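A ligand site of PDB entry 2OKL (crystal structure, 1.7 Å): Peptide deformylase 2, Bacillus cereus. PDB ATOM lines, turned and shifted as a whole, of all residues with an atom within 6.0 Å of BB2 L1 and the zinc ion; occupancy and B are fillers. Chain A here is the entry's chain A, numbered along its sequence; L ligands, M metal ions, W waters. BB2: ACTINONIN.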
ATOM      1  N   ARG A  57      21.665 -35.847 -18.380  1.00  0.00           N
ATOM      2  CA  ARG A  57      21.494 -34.406 -18.351  1.00  0.00           C
ATOM      3  C   ARG A  57      21.900 -33.952 -19.758  1.00  0.00           C
ATOM      4  O   ARG A  57      22.981 -34.277 -20.240  1.00  0.00           O
ATOM      5  CB  ARG A  57      22.409 -33.778 -17.301  1.00  0.00           C
ATOM      6  CG  ARG A  57      22.352 -32.250 -17.207  1.00  0.00           C
ATOM      7  CD  ARG A  57      23.261 -31.739 -16.082  1.00  0.00           C
ATOM      8  NE  ARG A  57      23.512 -30.302 -16.169  1.00  0.00           N
ATOM      9  CZ  ARG A  57      24.397 -29.654 -15.409  1.00  0.00           C
ATOM     10  NH1 ARG A  57      25.111 -30.308 -14.489  1.00  0.00           N
ATOM     11  NH2 ARG A  57      24.579 -28.352 -15.569  1.00  0.00           N
ATOM     12  N   PRO A  58      21.017 -33.223 -20.449  1.00  0.00           N
ATOM     13  CA  PRO A  58      21.296 -32.738 -21.796  1.00  0.00           C
ATOM     14  C   PRO A  58      22.533 -31.841 -21.823  1.00  0.00           C
ATOM     15  O   PRO A  58      22.710 -30.997 -20.942  1.00  0.00           O
ATOM     16  CB  PRO A  58      20.028 -31.971 -22.162  1.00  0.00           C
ATOM     17  CG  PRO A  58      18.964 -32.686 -21.384  1.00  0.00           C
ATOM     18  CD  PRO A  58      19.633 -32.890 -20.053  1.00  0.00           C
ATOM     19  N   GLY A  59      23.375 -32.046 -22.827  1.00  0.00           N
ATOM     20  CA  GLY A  59      24.596 -31.254 -22.969  1.00  0.00           C
ATOM     21  C   GLY A  59      24.968 -31.182 -24.440  1.00  0.00           C
ATOM     22  O   GLY A  59      24.442 -31.934 -25.250  1.00  0.00           O
ATOM     23  N   ILE A  60      25.880 -30.274 -24.783  1.00  0.00           N
ATOM     24  CA  ILE A  60      26.273 -30.131 -26.186  1.00  0.00           C
ATOM     25  C   ILE A  60      27.731 -30.449 -26.463  1.00  0.00           C
ATOM     26  O   ILE A  60      28.238 -30.156 -27.545  1.00  0.00           O
ATOM     27  CB  ILE A  60      25.944 -28.703 -26.685  1.00  0.00           C
ATOM     28  CG1 ILE A  60      26.562 -27.665 -25.759  1.00  0.00           C
ATOM     29  CG2 ILE A  60      24.435 -28.515 -26.752  1.00  0.00           C
ATOM     30  CD1 ILE A  60      26.237 -26.223 -26.158  1.00  0.00           C
ATOM     31  N   GLY A  61      28.398 -31.075 -25.504  1.00  0.00           N
ATOM     32  CA  GLY A  61      29.799 -31.441 -25.678  1.00  0.00           C
ATOM     33  C   GLY A  61      30.301 -32.245 -24.499  1.00  0.00           C
ATOM     34  O   GLY A  61      29.683 -32.251 -23.439  1.00  0.00           O
ATOM     35  N   LEU A  62      31.426 -32.928 -24.695  1.00  0.00           N
ATOM     36  CA  LEU A  62      32.007 -33.739 -23.636  1.00  0.00           C
ATOM     37  C   LEU A  62      33.501 -33.949 -23.869  1.00  0.00           C
ATOM     38  O   LEU A  62      33.945 -34.094 -25.020  1.00  0.00           O
ATOM     39  CB  LEU A  62      31.293 -35.090 -23.556  1.00  0.00           C
ATOM     40  CG  LEU A  62      31.700 -35.993 -22.391  1.00  0.00           C
ATOM     41  CD1 LEU A  62      31.242 -35.374 -21.091  1.00  0.00           C
ATOM     42  CD2 LEU A  62      31.091 -37.371 -22.562  1.00  0.00           C
ATOM     43  N   ALA A  63      34.273 -33.977 -22.787  1.00  0.00           N
ATOM     44  CA  ALA A  63      35.705 -34.201 -22.868  1.00  0.00           C
ATOM     45  C   ALA A  63      36.023 -35.505 -22.124  1.00  0.00           C
ATOM     46  O   ALA A  63      35.401 -35.816 -21.111  1.00  0.00           O
ATOM     47  CB  ALA A  63      36.460 -33.035 -22.240  1.00  0.00           C
ATOM     48  N   GLN A  66      36.352 -35.892 -18.328  1.00  0.00           N
ATOM     49  CA  GLN A  66      35.068 -35.872 -17.640  1.00  0.00           C
ATOM     50  C   GLN A  66      34.501 -37.265 -17.350  1.00  0.00           C
ATOM     51  O   GLN A  66      33.698 -37.424 -16.440  1.00  0.00           O
ATOM     52  CB  GLN A  66      34.044 -35.067 -18.431  1.00  0.00           C
ATOM     53  CG  GLN A  66      34.293 -33.585 -18.410  1.00  0.00           C
ATOM     54  CD  GLN A  66      33.224 -32.812 -19.140  1.00  0.00           C
ATOM     55  OE1 GLN A  66      33.161 -32.830 -20.369  1.00  0.00           O
ATOM     56  NE2 GLN A  66      32.366 -32.131 -18.387  1.00  0.00           N
ATOM     57  N   LEU A 105      28.433 -15.985 -23.689  1.00  0.00           N
ATOM     58  CA  LEU A 105      27.002 -16.190 -23.499  1.00  0.00           C
ATOM     59  C   LEU A 105      26.604 -15.281 -22.322  1.00  0.00           C
ATOM     60  O   LEU A 105      27.225 -15.309 -21.249  1.00  0.00           O
ATOM     61  CB  LEU A 105      26.727 -17.662 -23.160  1.00  0.00           C
ATOM     62  CG  LEU A 105      26.688 -18.661 -24.326  1.00  0.00           C
ATOM     63  CD1 LEU A 105      26.998 -20.078 -23.858  1.00  0.00           C
ATOM     64  CD2 LEU A 105      25.297 -18.606 -24.950  1.00  0.00           C
ATOM     65  N   GLY A 107      24.099 -15.533 -20.483  1.00  0.00           N
ATOM     66  CA  GLY A 107      23.560 -16.338 -19.409  1.00  0.00           C
ATOM     67  C   GLY A 107      24.611 -17.234 -18.774  1.00  0.00           C
ATOM     68  O   GLY A 107      24.285 -18.090 -17.940  1.00  0.00           O
ATOM     69  N   GLY A 108      25.868 -17.034 -19.161  1.00  0.00           N
ATOM     70  CA  GLY A 108      26.964 -17.819 -18.611  1.00  0.00           C
ATOM     71  C   GLY A 108      27.106 -19.220 -19.182  1.00  0.00           C
ATOM     72  O   GLY A 108      26.537 -19.542 -20.231  1.00  0.00           O
ATOM     73  N   GLU A 109      27.862 -20.062 -18.485  1.00  0.00           N
ATOM     74  CA  GLU A 109      28.078 -21.445 -18.898  1.00  0.00           C
ATOM     75  C   GLU A 109      27.859 -22.424 -17.760  1.00  0.00           C
ATOM     76  O   GLU A 109      28.037 -22.081 -16.586  1.00  0.00           O
ATOM     77  CB  GLU A 109      29.513 -21.621 -19.441  1.00  0.00           C
ATOM     78  CG  GLU A 109      29.743 -21.050 -20.831  1.00  0.00           C
ATOM     79  CD  GLU A 109      31.172 -21.273 -21.322  1.00  0.00           C
ATOM     80  OE1 GLU A 109      31.788 -22.303 -20.945  1.00  0.00           O
ATOM     81  OE2 GLU A 109      31.677 -20.440 -22.097  1.00  0.00           O
ATOM     82  N   GLY A 110      27.473 -23.639 -18.111  1.00  0.00           N
ATOM     83  CA  GLY A 110      27.261 -24.697 -17.141  1.00  0.00           C
ATOM     84  C   GLY A 110      28.189 -25.836 -17.544  1.00  0.00           C
ATOM     85  O   GLY A 110      28.683 -25.846 -18.672  1.00  0.00           O
ATOM     86  N   CYS A 111      28.426 -26.788 -16.644  1.00  0.00           N
ATOM     87  CA  CYS A 111      29.316 -27.907 -16.938  1.00  0.00           C
ATOM     88  C   CYS A 111      28.769 -29.175 -16.294  1.00  0.00           C
ATOM     89  O   CYS A 111      28.296 -29.157 -15.156  1.00  0.00           O
ATOM     90  CB  CYS A 111      30.736 -27.606 -16.401  1.00  0.00           C
ATOM     91  SG  CYS A 111      32.022 -28.854 -16.745  1.00  0.00           S
ATOM     92  N   LEU A 112      28.821 -30.278 -17.036  1.00  0.00           N
ATOM     93  CA  LEU A 112      28.343 -31.552 -16.523  1.00  0.00           C
ATOM     94  C   LEU A 112      29.126 -32.010 -15.303  1.00  0.00           C
ATOM     95  O   LEU A 112      28.611 -32.779 -14.490  1.00  0.00           O
ATOM     96  CB  LEU A 112      28.427 -32.615 -17.618  1.00  0.00           C
ATOM     97  CG  LEU A 112      27.134 -32.934 -18.387  1.00  0.00           C
ATOM     98  CD1 LEU A 112      26.528 -31.674 -18.984  1.00  0.00           C
ATOM     99  CD2 LEU A 112      27.445 -33.958 -19.467  1.00  0.00           C
ATOM    100  N   SER A 113      30.365 -31.541 -15.171  1.00  0.00           N
ATOM    101  CA  SER A 113      31.221 -31.912 -14.045  1.00  0.00           C
ATOM    102  C   SER A 113      31.068 -30.986 -12.843  1.00  0.00           C
ATOM    103  O   SER A 113      31.680 -31.215 -11.800  1.00  0.00           O
ATOM    104  CB  SER A 113      32.694 -31.896 -14.488  1.00  0.00           C
ATOM    105  OG  SER A 113      32.962 -32.879 -15.469  1.00  0.00           O
ATOM    106  N   ARG A 124      35.238 -15.821 -24.224  1.00  0.00           N
ATOM    107  CA  ARG A 124      35.718 -16.803 -25.198  1.00  0.00           C
ATOM    108  C   ARG A 124      36.142 -16.082 -26.468  1.00  0.00           C
ATOM    109  O   ARG A 124      35.612 -15.021 -26.777  1.00  0.00           O
ATOM    110  CB  ARG A 124      34.599 -17.776 -25.580  1.00  0.00           C
ATOM    111  CG  ARG A 124      34.045 -18.616 -24.454  1.00  0.00           C
ATOM    112  CD  ARG A 124      35.087 -19.568 -23.936  1.00  0.00           C
ATOM    113  NE  ARG A 124      34.527 -20.517 -22.985  1.00  0.00           N
ATOM    114  CZ  ARG A 124      35.264 -21.419 -22.345  1.00  0.00           C
ATOM    115  NH1 ARG A 124      36.567 -21.480 -22.551  1.00  0.00           N
ATOM    116  NH2 ARG A 124      34.698 -22.261 -21.499  1.00  0.00           N
ATOM    117  N   LEU A 147      28.590 -19.840 -30.949  1.00  0.00           N
ATOM    118  CA  LEU A 147      28.381 -20.950 -30.016  1.00  0.00           C
ATOM    119  C   LEU A 147      29.291 -22.150 -30.256  1.00  0.00           C
ATOM    120  O   LEU A 147      29.815 -22.715 -29.308  1.00  0.00           O
ATOM    121  CB  LEU A 147      26.903 -21.400 -30.025  1.00  0.00           C
ATOM    122  CG  LEU A 147      26.555 -22.434 -28.953  1.00  0.00           C
ATOM    123  CD1 LEU A 147      26.943 -21.909 -27.560  1.00  0.00           C
ATOM    124  CD2 LEU A 147      25.058 -22.732 -29.009  1.00  0.00           C
ATOM    125  N   ILE A 150      32.603 -21.509 -28.860  1.00  0.00           N
ATOM    126  CA  ILE A 150      32.535 -21.502 -27.398  1.00  0.00           C
ATOM    127  C   ILE A 150      32.581 -22.929 -26.855  1.00  0.00           C
ATOM    128  O   ILE A 150      33.345 -23.227 -25.942  1.00  0.00           O
ATOM    129  CB  ILE A 150      31.254 -20.804 -26.890  1.00  0.00           C
ATOM    130  CG1 ILE A 150      31.373 -19.296 -27.148  1.00  0.00           C
ATOM    131  CG2 ILE A 150      31.046 -21.080 -25.393  1.00  0.00           C
ATOM    132  CD1 ILE A 150      30.138 -18.479 -26.766  1.00  0.00           C
ATOM    133  N   VAL A 151      31.786 -23.815 -27.435  1.00  0.00           N
ATOM    134  CA  VAL A 151      31.756 -25.205 -26.983  1.00  0.00           C
ATOM    135  C   VAL A 151      33.136 -25.862 -27.174  1.00  0.00           C
ATOM    136  O   VAL A 151      33.596 -26.594 -26.297  1.00  0.00           O
ATOM    137  CB  VAL A 151      30.686 -26.020 -27.743  1.00  0.00           C
ATOM    138  CG1 VAL A 151      30.715 -27.490 -27.298  1.00  0.00           C
ATOM    139  CG2 VAL A 151      29.319 -25.413 -27.500  1.00  0.00           C
ATOM    140  N   HIS A 154      35.473 -24.698 -24.426  1.00  0.00           N
ATOM    141  CA  HIS A 154      35.105 -25.306 -23.152  1.00  0.00           C
ATOM    142  C   HIS A 154      35.631 -26.741 -23.086  1.00  0.00           C
ATOM    143  O   HIS A 154      36.229 -27.142 -22.076  1.00  0.00           O
ATOM    144  CB  HIS A 154      33.573 -25.296 -23.001  1.00  0.00           C
ATOM    145  CG  HIS A 154      33.070 -25.925 -21.734  1.00  0.00           C
ATOM    146  ND1 HIS A 154      32.505 -25.193 -20.717  1.00  0.00           N
ATOM    147  CD2 HIS A 154      33.034 -27.215 -21.326  1.00  0.00           C
ATOM    148  CE1 HIS A 154      32.136 -26.006 -19.745  1.00  0.00           C
ATOM    149  NE2 HIS A 154      32.445 -27.237 -20.086  1.00  0.00           N
ATOM    150  N   GLU A 155      35.422 -27.519 -24.150  1.00  0.00           N
ATOM    151  CA  GLU A 155      35.863 -28.905 -24.155  1.00  0.00           C
ATOM    152  C   GLU A 155      37.378 -29.048 -24.191  1.00  0.00           C
ATOM    153  O   GLU A 155      37.940 -29.904 -23.500  1.00  0.00           O
ATOM    154  CB  GLU A 155      35.261 -29.674 -25.334  1.00  0.00           C
ATOM    155  CG  GLU A 155      33.736 -29.744 -25.349  1.00  0.00           C
ATOM    156  CD  GLU A 155      33.120 -30.040 -23.996  1.00  0.00           C
ATOM    157  OE1 GLU A 155      33.792 -30.629 -23.109  1.00  0.00           O
ATOM    158  OE2 GLU A 155      31.939 -29.684 -23.815  1.00  0.00           O
ATOM    159  N   HIS A 158      39.014 -28.447 -20.867  1.00  0.00           N
ATOM    160  CA  HIS A 158      38.985 -29.638 -20.033  1.00  0.00           C
ATOM    161  C   HIS A 158      40.226 -30.498 -20.223  1.00  0.00           C
ATOM    162  O   HIS A 158      40.710 -31.129 -19.281  1.00  0.00           O
ATOM    163  CB  HIS A 158      37.752 -30.490 -20.348  1.00  0.00           C
ATOM    164  CG  HIS A 158      36.530 -30.101 -19.577  1.00  0.00           C
ATOM    165  ND1 HIS A 158      36.512 -30.025 -18.199  1.00  0.00           N
ATOM    166  CD2 HIS A 158      35.276 -29.803 -19.983  1.00  0.00           C
ATOM    167  CE1 HIS A 158      35.297 -29.705 -17.795  1.00  0.00           C
ATOM    168  NE2 HIS A 158      34.522 -29.554 -18.852  1.00  0.00           N
ATOM    169  N   PHE A 164      35.491 -23.868 -16.684  1.00  0.00           N
ATOM    170  CA  PHE A 164      34.870 -22.652 -17.180  1.00  0.00           C
ATOM    171  C   PHE A 164      34.932 -21.474 -16.221  1.00  0.00           C
ATOM    172  O   PHE A 164      35.218 -20.350 -16.625  1.00  0.00           O
ATOM    173  CB  PHE A 164      33.423 -22.934 -17.617  1.00  0.00           C
ATOM    174  CG  PHE A 164      32.424 -22.924 -16.492  1.00  0.00           C
ATOM    175  CD1 PHE A 164      31.806 -21.738 -16.105  1.00  0.00           C
ATOM    176  CD2 PHE A 164      32.072 -24.099 -15.854  1.00  0.00           C
ATOM    177  CE1 PHE A 164      30.846 -21.728 -15.081  1.00  0.00           C
ATOM    178  CE2 PHE A 164      31.109 -24.109 -14.829  1.00  0.00           C
ATOM    179  CZ  PHE A 164      30.503 -22.914 -14.443  1.00  0.00           C
HETATM  180  C5  BB2 L   1      28.835 -29.931 -21.307  1.00  0.00           C
HETATM  181  C3  BB2 L   1      30.218 -30.044 -20.641  1.00  0.00           C
HETATM  182  O4  BB2 L   1      30.248 -29.970 -19.393  1.00  0.00           O
HETATM  183  N1  BB2 L   1      31.302 -30.190 -21.380  1.00  0.00           N
HETATM  184  O2  BB2 L   1      32.433 -30.287 -20.922  1.00  0.00           O
HETATM  185  C6  BB2 L   1      28.453 -28.404 -21.359  1.00  0.00           C
HETATM  186  C12 BB2 L   1      26.952 -28.082 -21.572  1.00  0.00           C
HETATM  187  O13 BB2 L   1      26.275 -28.604 -22.440  1.00  0.00           O
HETATM  188  C7  BB2 L   1      29.289 -27.778 -22.539  1.00  0.00           C
HETATM  189  C8  BB2 L   1      28.986 -26.264 -22.632  1.00  0.00           C
HETATM  190  C9  BB2 L   1      29.761 -25.574 -23.725  1.00  0.00           C
HETATM  191  C10 BB2 L   1      29.853 -24.068 -23.462  1.00  0.00           C
HETATM  192  C11 BB2 L   1      28.603 -23.321 -23.778  1.00  0.00           C
HETATM  193  N14 BB2 L   1      26.458 -27.186 -20.723  1.00  0.00           N
HETATM  194  C15 BB2 L   1      25.127 -26.596 -20.760  1.00  0.00           C
HETATM  195  C16 BB2 L   1      24.272 -26.934 -19.492  1.00  0.00           C
HETATM  196  C18 BB2 L   1      24.424 -28.391 -19.079  1.00  0.00           C
HETATM  197  C17 BB2 L   1      22.806 -26.641 -19.794  1.00  0.00           C
HETATM  198  C19 BB2 L   1      25.339 -25.077 -20.930  1.00  0.00           C
HETATM  199  O20 BB2 L   1      26.094 -24.491 -20.166  1.00  0.00           O
HETATM  200  N21 BB2 L   1      24.694 -24.436 -21.921  1.00  0.00           N
HETATM  201  C22 BB2 L   1      24.845 -22.992 -22.157  1.00  0.00           C
HETATM  202  C23 BB2 L   1      23.759 -25.069 -22.910  1.00  0.00           C
HETATM  203  C24 BB2 L   1      23.327 -23.926 -23.776  1.00  0.00           C
HETATM  204  C25 BB2 L   1      24.350 -22.838 -23.598  1.00  0.00           C
HETATM  205  C26 BB2 L   1      24.029 -22.096 -21.204  1.00  0.00           C
HETATM  206  O27 BB2 L   1      24.265 -20.847 -21.242  1.00  0.00           O
HETATM  207  C5  BB2 L   2      19.274 -10.723 -26.423  1.00  0.00           C
HETATM  208  C3  BB2 L   2      19.841 -10.206 -27.735  1.00  0.00           C
HETATM  209  O4  BB2 L   2      20.239  -9.029 -27.733  1.00  0.00           O
HETATM  210  N1  BB2 L   2      19.876 -10.969 -28.813  1.00  0.00           N
HETATM  211  O2  BB2 L   2      20.321 -10.616 -29.906  1.00  0.00           O
HETATM  212  C6  BB2 L   2      20.186 -11.886 -25.844  1.00  0.00           C
HETATM  213  C12 BB2 L   2      19.942 -13.295 -26.459  1.00  0.00           C
HETATM  214  O13 BB2 L   2      18.813 -13.780 -26.592  1.00  0.00           O
HETATM  215  C7  BB2 L   2      19.830 -11.917 -24.316  1.00  0.00           C
HETATM  216  C8  BB2 L   2      20.624 -12.994 -23.549  1.00  0.00           C
HETATM  217  C9  BB2 L   2      20.244 -12.983 -22.072  1.00  0.00           C
HETATM  218  C10 BB2 L   2      20.400 -14.350 -21.424  1.00  0.00           C
HETATM  219  C11 BB2 L   2      20.349 -14.294 -19.934  1.00  0.00           C
HETATM  220  N14 BB2 L   2      21.037 -13.960 -26.816  1.00  0.00           N
HETATM  221  C15 BB2 L   2      21.049 -15.358 -27.275  1.00  0.00           C
HETATM  222  C16 BB2 L   2      22.203 -15.717 -28.256  1.00  0.00           C
HETATM  223  C18 BB2 L   2      22.457 -17.205 -28.415  1.00  0.00           C
HETATM  224  C17 BB2 L   2      23.468 -15.003 -27.786  1.00  0.00           C
HETATM  225  C19 BB2 L   2      21.024 -16.256 -25.993  1.00  0.00           C
HETATM  226  O20 BB2 L   2      21.856 -16.068 -25.103  1.00  0.00           O
HETATM  227  N21 BB2 L   2      20.074 -17.200 -25.908  1.00  0.00           N
HETATM  228  C22 BB2 L   2      19.948 -18.090 -24.756  1.00  0.00           C
HETATM  229  C23 BB2 L   2      19.026 -17.486 -26.952  1.00  0.00           C
HETATM  230  C24 BB2 L   2      18.223 -18.630 -26.379  1.00  0.00           C
HETATM  231  C25 BB2 L   2      18.540 -18.688 -24.919  1.00  0.00           C
HETATM  232  C26 BB2 L   2      21.007 -19.185 -24.693  1.00  0.00           C
HETATM  233  O27 BB2 L   2      21.109 -19.816 -23.605  1.00  0.00           O
HETATM  234 ZN    ZN M   1      32.394 -29.023 -19.065  1.00  0.00          ZN
HETATM  235  O   HOH W   1      22.201 -18.933 -21.307  1.00  0.00           O
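Water W1 lies within hydrogen-bond range of an oxygen (O27) of BB2 L2 (2.7 Å) and an oxygen (O27) of BB2 L1 (2.8 Å).
NH2 of Arg 57 touches C18 of BB2 L1, at 3.5 Å.
O of Pro 58 touches C18 of BB2 L1, 3.6 Å away.
CA of Gly 59 touches O13 of BB2 L1, 3.2 Å away.
CD1 of Leu 105 touches C11 of BB2 L1, at 3.6 Å.
Glu 109 touches BB2 L1 (C to O20, 3.6 Å).
Ile 150 touches BB2 L1.
CG2 of Val 151 touches C9 of BB2 L1, 3.8 Å away.
Hydrophobic or aromatic side chains that line BB2 L1: Ile 60, Leu 105, Leu 112, Ile 150, Val 151, His 154 and His 158.
Within 4 Å of BB2 L1: Arg 57, Pro 58, Gly 59, Ile 60, Gly 61, Gln 66, Leu 105, Gly 108, Glu 109, Gly 110, Cys 111, Leu 112, Ile 150, Val 151, His 154, Glu 155 and His 158.
Along chain A the residues within 4 Å of BB2 L1 span positions 57 to 158.
The nearest printed residue that does not touch BB2 L1 is Leu 62 (4.3 Å).
Merely in contact with the zinc ion: Gln 66 (3.2 Å).
Four residues have an atom within 4 Å of the zinc ion: Gln 66, Cys 111, His 154 and His 158.
The zinc ion is bound by NE2 of His 154 (2.1 Å), NE2 of His 158 (2.2 Å), O2 of BB2 L1 (2.2 Å), SG of Cys 111 (2.4 Å) and O4 of BB2 L1 (2.4 Å).
The zinc ion has five donor atoms within binding distance.
An oxygen (O13) of BB2 L1 sits at hydrogen-bond distance from the backbone NH (N) of Ile 60, 2.9 Å away.
The backbone carbonyl oxygen of Gly 61 lies close to a nitrogen (N1) of BB2 L1.
N of Gly 110 sits at hydrogen-bond distance from O20 of BB2 L1 (2.6 Å).
OE2 of Glu 155 sits at hydrogen-bond distance from N1 of BB2 L1 (2.6 Å).
O of Gly 108 sits at hydrogen-bond distance from O27 of BB2 L1.
OE1 of Gln 66 sits at hydrogen-bond distance from N1 of BB2 L1.
An oxygen (O4) of BB2 L1 lies close to the backbone NH (N) of Leu 112.
A nitrogen (N14) of BB2 L1 sits at hydrogen-bond distance from the backbone carbonyl oxygen of Gly 110.
OE1 of Glu 155 is in hydrogen-bond range of N of Ala 63, at 3.4 Å.
The side-chain amide oxygen of Gln 66 sits at hydrogen-bond distance from the backbone NH of Ala 63, 2.9 Å away.
The side-chain sulfur (SG) of Cys 111 sits close to the backbone NH (N) of Ser 113 (3.5 Å).
A ring nitrogen (ND1) of His 154 sits at hydrogen-bond distance from the side-chain carboxylate (OE1) of Glu 109, at 3.0 Å.
The side-chain hydroxyl of Ser 113 sits at hydrogen-bond distance from the side-chain amide nitrogen of Gln 66, 3.1 Å away.
The side-chain amide nitrogen of Gln 66 lies close to a ring nitrogen (NE2) of His 158 (3.4 Å).
The backbone carbonyl oxygen (O) of Cys 111 lies within hydrogen-bond range of the guanidinium group (NH1) of Arg 57 (3.5 Å).
The backbone NH (N) of Leu 62 lies within hydrogen-bond range of the side-chain carboxylate (OE2) of Glu 155.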
